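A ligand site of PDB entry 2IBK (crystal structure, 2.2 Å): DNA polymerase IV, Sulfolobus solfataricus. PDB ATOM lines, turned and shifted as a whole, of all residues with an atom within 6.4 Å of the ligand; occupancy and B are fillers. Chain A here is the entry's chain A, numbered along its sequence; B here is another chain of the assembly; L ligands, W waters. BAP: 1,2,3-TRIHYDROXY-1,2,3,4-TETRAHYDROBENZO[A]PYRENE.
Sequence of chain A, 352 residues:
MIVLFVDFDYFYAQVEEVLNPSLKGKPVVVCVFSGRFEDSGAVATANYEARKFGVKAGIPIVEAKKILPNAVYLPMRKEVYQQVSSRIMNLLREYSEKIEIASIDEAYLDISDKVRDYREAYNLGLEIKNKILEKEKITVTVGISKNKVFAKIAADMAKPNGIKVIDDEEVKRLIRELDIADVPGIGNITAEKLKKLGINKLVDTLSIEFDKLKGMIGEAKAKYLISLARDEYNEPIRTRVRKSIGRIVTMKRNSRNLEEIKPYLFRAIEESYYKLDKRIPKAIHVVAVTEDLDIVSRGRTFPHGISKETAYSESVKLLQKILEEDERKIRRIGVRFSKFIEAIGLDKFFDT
The side-chain amino group (NZ) of Lys 275 is in hydrogen-bond range of an oxygen (O3') of the ligand (3.0 Å). The side-chain amino group (NZ) of Lys 78 lies within hydrogen-bond range of an oxygen (O2') of the ligand. N2 of DG 5 of chain B is covalently linked to a carbon (C4') of the ligand, 1.4 Å away.
The side-chain amino group (NZ) of Lys 275 lies within salt-bridge range of OP1 of DA 6 of chain B (3.6 Å). The guanidinium group (NH1) of Arg 247 lies within salt-bridge range of OP1 of DA 6 of chain B (3.1 Å). OP1 of DA 7 of chain B is in salt-bridge range of NZ of Lys 275 (3.3 Å). OP2 of DG 5 of chain B lies within salt-bridge range of the side-chain amino group (NZ) of Lys 78, 2.7 Å away. NZ of Lys 275 is in hydrogen-bond range of O of Gly 246 (2.8 Å). The guanidinium group (NE) of Arg 247 is in salt-bridge range of the side-chain carboxylate (OE1) of Glu 271, 2.8 Å away. N1 of DG 5 of chain B lies close to the side-chain carboxylate (OE1) of Glu 79, at 2.6 Å.
Glu 79 touches the ligand. Arg 247 touches the ligand (NE to C4, 3.3 Å). CD of Glu 271 touches C3 of the ligand (3.6 Å). Tyr 274 touches the ligand. DA 6 of chain B touches the ligand (OP1 to O3', 3.9 Å). Hydrophobic or aromatic side chains that line the ligand: Tyr 274. Eight residues have an atom within 4 Å of the ligand: Lys 78, Glu 79, Arg 247, Glu 271, Tyr 274, Lys 275, DG 5 of chain B and DA 6 of chain B. Along chain A the residues within 4 Å of the ligand span positions 78 to 275.
Water W1 bridges O2' of the ligand (2.7 Å) and OE1 of Gln 82 (2.9 Å). Water W2 bridges an oxygen (O1') of the ligand and the side-chain carboxylate of Glu 79.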
ATOM      1  N   MET A  76      22.231  -6.665  14.192  1.00  0.00           N
ATOM      2  CA  MET A  76      22.259  -7.871  14.989  1.00  0.00           C
ATOM      3  C   MET A  76      21.486  -7.697  16.292  1.00  0.00           C
ATOM      4  O   MET A  76      21.682  -6.725  17.013  1.00  0.00           O
ATOM      5  CB  MET A  76      23.707  -8.260  15.313  1.00  0.00           C
ATOM      6  CG  MET A  76      23.818  -9.546  16.122  1.00  0.00           C
ATOM      7  SD  MET A  76      25.489  -9.867  16.674  1.00  0.00           S
ATOM      8  CE  MET A  76      25.727  -8.518  17.755  1.00  0.00           C
ATOM      9  N   LYS A  78      21.437  -9.843  19.078  1.00  0.00           N
ATOM     10  CA  LYS A  78      22.011 -10.947  19.816  1.00  0.00           C
ATOM     11  C   LYS A  78      21.121 -11.573  20.890  1.00  0.00           C
ATOM     12  O   LYS A  78      20.988 -12.795  20.953  1.00  0.00           O
ATOM     13  CB  LYS A  78      23.354 -10.506  20.419  1.00  0.00           C
ATOM     14  CG  LYS A  78      24.199 -11.631  20.965  1.00  0.00           C
ATOM     15  CD  LYS A  78      24.533 -12.649  19.915  1.00  0.00           C
ATOM     16  CE  LYS A  78      25.386 -13.762  20.500  1.00  0.00           C
ATOM     17  NZ  LYS A  78      26.652 -13.225  21.058  1.00  0.00           N
ATOM     18  N   GLU A  79      20.520 -10.729  21.718  1.00  0.00           N
ATOM     19  CA  GLU A  79      19.654 -11.193  22.805  1.00  0.00           C
ATOM     20  C   GLU A  79      18.533 -12.086  22.300  1.00  0.00           C
ATOM     21  O   GLU A  79      18.225 -13.101  22.899  1.00  0.00           O
ATOM     22  CB  GLU A  79      19.088 -10.015  23.579  1.00  0.00           C
ATOM     23  CG  GLU A  79      20.099  -9.358  24.522  1.00  0.00           C
ATOM     24  CD  GLU A  79      21.394  -8.963  23.831  1.00  0.00           C
ATOM     25  OE1 GLU A  79      21.322  -8.327  22.751  1.00  0.00           O
ATOM     26  OE2 GLU A  79      22.477  -9.288  24.360  1.00  0.00           O
ATOM     27  N   GLN A  82      20.050 -15.386  21.164  1.00  0.00           N
ATOM     28  CA  GLN A  82      20.493 -16.170  22.309  1.00  0.00           C
ATOM     29  C   GLN A  82      19.328 -16.918  22.964  1.00  0.00           C
ATOM     30  O   GLN A  82      19.473 -18.065  23.388  1.00  0.00           O
ATOM     31  CB  GLN A  82      21.172 -15.273  23.335  1.00  0.00           C
ATOM     32  CG  GLN A  82      21.630 -15.998  24.584  1.00  0.00           C
ATOM     33  CD  GLN A  82      22.687 -17.061  24.301  1.00  0.00           C
ATOM     34  OE1 GLN A  82      23.817 -16.734  23.952  1.00  0.00           O
ATOM     35  NE2 GLN A  82      22.317 -18.328  24.452  1.00  0.00           N
ATOM     36  N   GLY A 246      33.629  -9.739  28.222  1.00  0.00           N
ATOM     37  CA  GLY A 246      34.082  -8.381  28.068  1.00  0.00           C
ATOM     38  C   GLY A 246      33.148  -7.456  27.340  1.00  0.00           C
ATOM     39  O   GLY A 246      32.070  -7.830  26.907  1.00  0.00           O
ATOM     40  N   ARG A 247      33.588  -6.217  27.198  1.00  0.00           N
ATOM     41  CA  ARG A 247      32.800  -5.201  26.537  1.00  0.00           C
ATOM     42  C   ARG A 247      33.793  -4.306  25.841  1.00  0.00           C
ATOM     43  O   ARG A 247      34.718  -3.784  26.453  1.00  0.00           O
ATOM     44  CB  ARG A 247      32.005  -4.403  27.579  1.00  0.00           C
ATOM     45  CG  ARG A 247      30.925  -3.537  27.005  1.00  0.00           C
ATOM     46  CD  ARG A 247      29.653  -4.328  26.724  1.00  0.00           C
ATOM     47  NE  ARG A 247      28.672  -3.470  26.072  1.00  0.00           N
ATOM     48  CZ  ARG A 247      28.721  -3.113  24.788  1.00  0.00           C
ATOM     49  NH1 ARG A 247      29.705  -3.550  24.019  1.00  0.00           N
ATOM     50  NH2 ARG A 247      27.802  -2.297  24.291  1.00  0.00           N
ATOM     51  N   GLU A 270      31.002  -0.880  33.417  1.00  0.00           N
ATOM     52  CA  GLU A 270      29.646  -0.848  33.952  1.00  0.00           C
ATOM     53  C   GLU A 270      28.750  -1.859  33.242  1.00  0.00           C
ATOM     54  O   GLU A 270      27.915  -2.496  33.877  1.00  0.00           O
ATOM     55  CB  GLU A 270      29.060   0.560  33.793  1.00  0.00           C
ATOM     56  CG  GLU A 270      27.771   0.780  34.566  1.00  0.00           C
ATOM     57  CD  GLU A 270      27.965   0.659  36.060  1.00  0.00           C
ATOM     58  OE1 GLU A 270      28.329  -0.439  36.531  1.00  0.00           O
ATOM     59  OE2 GLU A 270      27.764   1.666  36.771  1.00  0.00           O
ATOM     60  N   GLU A 271      28.922  -2.004  31.936  1.00  0.00           N
ATOM     61  CA  GLU A 271      28.127  -2.933  31.149  1.00  0.00           C
ATOM     62  C   GLU A 271      28.669  -4.353  31.246  1.00  0.00           C
ATOM     63  O   GLU A 271      27.905  -5.317  31.140  1.00  0.00           O
ATOM     64  CB  GLU A 271      28.057  -2.478  29.697  1.00  0.00           C
ATOM     65  CG  GLU A 271      27.721  -0.996  29.557  1.00  0.00           C
ATOM     66  CD  GLU A 271      27.466  -0.568  28.120  1.00  0.00           C
ATOM     67  OE1 GLU A 271      28.212  -1.011  27.222  1.00  0.00           O
ATOM     68  OE2 GLU A 271      26.530   0.227  27.893  1.00  0.00           O
ATOM     69  N   SER A 272      29.978  -4.475  31.451  1.00  0.00           N
ATOM     70  CA  SER A 272      30.592  -5.798  31.588  1.00  0.00           C
ATOM     71  C   SER A 272      30.093  -6.448  32.866  1.00  0.00           C
ATOM     72  O   SER A 272      29.793  -7.644  32.897  1.00  0.00           O
ATOM     73  CB  SER A 272      32.118  -5.674  31.672  1.00  0.00           C
ATOM     74  OG  SER A 272      32.673  -5.174  30.477  1.00  0.00           O
ATOM     75  N   TYR A 274      27.306  -6.130  34.256  1.00  0.00           N
ATOM     76  CA  TYR A 274      25.960  -6.600  34.065  1.00  0.00           C
ATOM     77  C   TYR A 274      26.054  -7.917  33.277  1.00  0.00           C
ATOM     78  O   TYR A 274      25.367  -8.875  33.605  1.00  0.00           O
ATOM     79  CB  TYR A 274      25.101  -5.553  33.323  1.00  0.00           C
ATOM     80  CG  TYR A 274      23.631  -5.905  33.155  1.00  0.00           C
ATOM     81  CD1 TYR A 274      22.675  -4.904  32.945  1.00  0.00           C
ATOM     82  CD2 TYR A 274      23.183  -7.240  33.143  1.00  0.00           C
ATOM     83  CE1 TYR A 274      21.329  -5.203  32.740  1.00  0.00           C
ATOM     84  CE2 TYR A 274      21.834  -7.550  32.929  1.00  0.00           C
ATOM     85  CZ  TYR A 274      20.913  -6.531  32.732  1.00  0.00           C
ATOM     86  OH  TYR A 274      19.569  -6.819  32.535  1.00  0.00           O
ATOM     87  N   LYS A 275      26.899  -7.990  32.248  1.00  0.00           N
ATOM     88  CA  LYS A 275      26.972  -9.266  31.543  1.00  0.00           C
ATOM     89  C   LYS A 275      27.672 -10.338  32.337  1.00  0.00           C
ATOM     90  O   LYS A 275      27.541 -11.519  32.029  1.00  0.00           O
ATOM     91  CB  LYS A 275      27.569  -9.148  30.126  1.00  0.00           C
ATOM     92  CG  LYS A 275      28.796  -8.309  29.932  1.00  0.00           C
ATOM     93  CD  LYS A 275      29.053  -8.109  28.439  1.00  0.00           C
ATOM     94  CE  LYS A 275      29.175  -9.434  27.698  1.00  0.00           C
ATOM     95  NZ  LYS A 275      29.764  -9.281  26.321  1.00  0.00           N
ATOM     96  N   LEU A 276      28.400  -9.941  33.383  1.00  0.00           N
ATOM     97  CA  LEU A 276      29.063 -10.922  34.238  1.00  0.00           C
ATOM     98  C   LEU A 276      27.949 -11.728  34.878  1.00  0.00           C
ATOM     99  O   LEU A 276      28.096 -12.919  35.172  1.00  0.00           O
ATOM    100  CB  LEU A 276      29.900 -10.220  35.321  1.00  0.00           C
ATOM    101  CG  LEU A 276      31.304  -9.811  34.894  1.00  0.00           C
ATOM    102  CD1 LEU A 276      31.907  -8.828  35.886  1.00  0.00           C
ATOM    103  CD2 LEU A 276      32.169 -11.058  34.774  1.00  0.00           C
ATOM    104  P    DT B   4      32.174  -5.518  17.751  1.00  0.00           P
ATOM    105  OP1  DT B   4      30.908  -5.204  18.471  1.00  0.00           O
ATOM    106  OP2  DT B   4      33.480  -5.405  18.458  1.00  0.00           O
ATOM    107  O5'  DT B   4      32.032  -6.986  17.193  1.00  0.00           O
ATOM    108  C5'  DT B   4      31.967  -8.072  18.069  1.00  0.00           C
ATOM    109  C4'  DT B   4      31.450  -9.291  17.346  1.00  0.00           C
ATOM    110  O4'  DT B   4      32.328  -9.629  16.241  1.00  0.00           O
ATOM    111  C3'  DT B   4      31.426 -10.509  18.266  1.00  0.00           C
ATOM    112  O3'  DT B   4      30.144 -11.090  18.235  1.00  0.00           O
ATOM    113  C2'  DT B   4      32.583 -11.369  17.815  1.00  0.00           C
ATOM    114  C1'  DT B   4      32.795 -10.956  16.364  1.00  0.00           C
ATOM    115  N1   DT B   4      34.210 -10.975  15.919  1.00  0.00           N
ATOM    116  C2   DT B   4      34.692 -12.141  15.363  1.00  0.00           C
ATOM    117  O2   DT B   4      34.042 -13.165  15.302  1.00  0.00           O
ATOM    118  N3   DT B   4      35.982 -12.068  14.893  1.00  0.00           N
ATOM    119  C4   DT B   4      36.824 -10.977  14.944  1.00  0.00           C
ATOM    120  O4   DT B   4      37.945 -11.058  14.446  1.00  0.00           O
ATOM    121  C5   DT B   4      36.278  -9.793  15.592  1.00  0.00           C
ATOM    122  C7   DT B   4      37.147  -8.582  15.760  1.00  0.00           C
ATOM    123  C6   DT B   4      35.007  -9.852  16.037  1.00  0.00           C
ATOM    124  P    DG B   5      29.238 -11.039  19.573  1.00  0.00           P
ATOM    125  OP1  DG B   5      30.154 -11.629  20.583  1.00  0.00           O
ATOM    126  OP2  DG B   5      27.984 -11.687  19.226  1.00  0.00           O
ATOM    127  O5'  DG B   5      28.994  -9.578  20.213  1.00  0.00           O
ATOM    128  C5'  DG B   5      28.183  -8.559  19.648  1.00  0.00           C
ATOM    129  C4'  DG B   5      28.908  -7.243  19.794  1.00  0.00           C
ATOM    130  O4'  DG B   5      28.281  -6.355  18.859  1.00  0.00           O
ATOM    131  C3'  DG B   5      28.957  -6.549  21.178  1.00  0.00           C
ATOM    132  O3'  DG B   5      30.340  -6.164  21.471  1.00  0.00           O
ATOM    133  C2'  DG B   5      28.159  -5.274  20.957  1.00  0.00           C
ATOM    134  C1'  DG B   5      27.690  -5.268  19.503  1.00  0.00           C
ATOM    135  N9   DG B   5      26.256  -5.463  19.418  1.00  0.00           N
ATOM    136  C8   DG B   5      25.447  -4.963  18.446  1.00  0.00           C
ATOM    137  N7   DG B   5      24.191  -5.276  18.592  1.00  0.00           N
ATOM    138  C5   DG B   5      24.167  -6.045  19.751  1.00  0.00           C
ATOM    139  C6   DG B   5      23.071  -6.650  20.392  1.00  0.00           C
ATOM    140  O6   DG B   5      21.919  -6.631  20.053  1.00  0.00           O
ATOM    141  N1   DG B   5      23.447  -7.343  21.552  1.00  0.00           N
ATOM    142  C2   DG B   5      24.726  -7.434  22.026  1.00  0.00           C
ATOM    143  N2   DG B   5      24.879  -8.154  23.168  1.00  0.00           N
ATOM    144  N3   DG B   5      25.784  -6.861  21.425  1.00  0.00           N
ATOM    145  C4   DG B   5      25.421  -6.186  20.295  1.00  0.00           C
ATOM    146  P    DA B   6      31.050  -6.536  22.890  1.00  0.00           P
ATOM    147  OP1  DA B   6      30.044  -6.600  23.980  1.00  0.00           O
ATOM    148  OP2  DA B   6      32.262  -5.687  23.075  1.00  0.00           O
ATOM    149  O5'  DA B   6      31.565  -8.009  22.638  1.00  0.00           O
ATOM    150  C5'  DA B   6      32.552  -8.288  21.641  1.00  0.00           C
ATOM    151  C4'  DA B   6      32.773  -9.776  21.598  1.00  0.00           C
ATOM    152  O4'  DA B   6      33.671 -10.173  20.535  1.00  0.00           O
ATOM    153  C3'  DA B   6      33.344 -10.336  22.895  1.00  0.00           C
ATOM    154  O3'  DA B   6      32.548 -11.422  23.336  1.00  0.00           O
ATOM    155  C2'  DA B   6      34.755 -10.773  22.515  1.00  0.00           C
ATOM    156  C1'  DA B   6      34.616 -11.093  21.027  1.00  0.00           C
ATOM    157  N9   DA B   6      35.857 -10.922  20.262  1.00  0.00           N
ATOM    158  C8   DA B   6      36.705  -9.853  20.303  1.00  0.00           C
ATOM    159  N7   DA B   6      37.748  -9.966  19.506  1.00  0.00           N
ATOM    160  C5   DA B   6      37.559 -11.200  18.907  1.00  0.00           C
ATOM    161  C6   DA B   6      38.320 -11.914  17.956  1.00  0.00           C
ATOM    162  N6   DA B   6      39.476 -11.485  17.441  1.00  0.00           N
ATOM    163  N1   DA B   6      37.853 -13.115  17.559  1.00  0.00           N
ATOM    164  C2   DA B   6      36.707 -13.564  18.084  1.00  0.00           C
ATOM    165  N3   DA B   6      35.906 -12.993  18.982  1.00  0.00           N
ATOM    166  C4   DA B   6      36.399 -11.798  19.355  1.00  0.00           C
ATOM    167  P    DA B   7      32.585 -11.864  24.885  1.00  0.00           P
ATOM    168  OP1  DA B   7      31.197 -12.120  25.347  1.00  0.00           O
ATOM    169  OP2  DA B   7      33.437 -10.887  25.606  1.00  0.00           O
ATOM    170  O5'  DA B   7      33.324 -13.255  24.800  1.00  0.00           O
ATOM    171  C5'  DA B   7      32.980 -14.170  23.775  1.00  0.00           C
ATOM    172  C4'  DA B   7      34.080 -15.179  23.581  1.00  0.00           C
ATOM    173  O4'  DA B   7      35.093 -14.675  22.658  1.00  0.00           O
ATOM    174  C3'  DA B   7      34.811 -15.589  24.856  1.00  0.00           C
ATOM    175  O3'  DA B   7      34.636 -16.985  25.053  1.00  0.00           O
ATOM    176  C2'  DA B   7      36.255 -15.186  24.606  1.00  0.00           C
ATOM    177  C1'  DA B   7      36.366 -15.124  23.081  1.00  0.00           C
ATOM    178  N9   DA B   7      37.377 -14.181  22.571  1.00  0.00           N
ATOM    179  C8   DA B   7      37.674 -12.939  23.078  1.00  0.00           C
ATOM    180  N7   DA B   7      38.649 -12.339  22.450  1.00  0.00           N
ATOM    181  C5   DA B   7      39.021 -13.224  21.453  1.00  0.00           C
ATOM    182  C6   DA B   7      40.020 -13.171  20.447  1.00  0.00           C
ATOM    183  N6   DA B   7      40.834 -12.132  20.262  1.00  0.00           N
ATOM    184  N1   DA B   7      40.142 -14.232  19.623  1.00  0.00           N
ATOM    185  C2   DA B   7      39.293 -15.251  19.772  1.00  0.00           C
ATOM    186  N3   DA B   7      38.311 -15.409  20.661  1.00  0.00           N
ATOM    187  C4   DA B   7      38.230 -14.362  21.499  1.00  0.00           C
HETATM  188  C1  BAP L   1      24.380  -4.037  29.548  1.00  0.00           C
HETATM  189  C2  BAP L   1      24.585  -2.900  28.733  1.00  0.00           C
HETATM  190  C3  BAP L   1      24.992  -3.057  27.375  1.00  0.00           C
HETATM  191  C3A BAP L   1      25.197  -4.331  26.838  1.00  0.00           C
HETATM  192  C4  BAP L   1      25.590  -4.483  25.512  1.00  0.00           C
HETATM  193  C5  BAP L   1      25.776  -5.773  24.991  1.00  0.00           C
HETATM  194  C5A BAP L   1      25.565  -6.922  25.787  1.00  0.00           C
HETATM  195  C6  BAP L   1      25.730  -8.219  25.270  1.00  0.00           C
HETATM  196  C7  BAP L   1      25.476  -9.367  26.115  1.00  0.00           C
HETATM  197  C8  BAP L   1      25.176  -9.163  27.460  1.00  0.00           C
HETATM  198  C8A BAP L   1      24.996  -7.895  27.972  1.00  0.00           C
HETATM  199  C9  BAP L   1      24.606  -7.732  29.306  1.00  0.00           C
HETATM  200  C10 BAP L   1      24.400  -6.440  29.821  1.00  0.00           C
HETATM  201  C1A BAP L   1      24.586  -5.319  29.022  1.00  0.00           C
HETATM  202  C3B BAP L   1      24.983  -5.476  27.665  1.00  0.00           C
HETATM  203  C5B BAP L   1      25.189  -6.758  27.140  1.00  0.00           C
HETATM  204  C1' BAP L   1      25.653 -10.749  25.674  1.00  0.00           C
HETATM  205  O1' BAP L   1      24.711 -11.638  26.187  1.00  0.00           O
HETATM  206  C2' BAP L   1      25.818 -10.867  24.133  1.00  0.00           C
HETATM  207  O2' BAP L   1      26.235 -12.158  23.762  1.00  0.00           O
HETATM  208  C3' BAP L   1      26.659  -9.787  23.480  1.00  0.00           C
HETATM  209  O3' BAP L   1      27.978  -9.945  23.942  1.00  0.00           O
HETATM  210  C4' BAP L   1      26.137  -8.372  23.850  1.00  0.00           C
HETATM  211  O   HOH W   1      24.161 -13.883  24.013  1.00  0.00           O
HETATM  212  O   HOH W   2      21.910 -12.655  25.127  1.00  0.00           O
HETATM  213  O   HOH W   3      29.346 -11.881  23.009  1.00  0.00           O
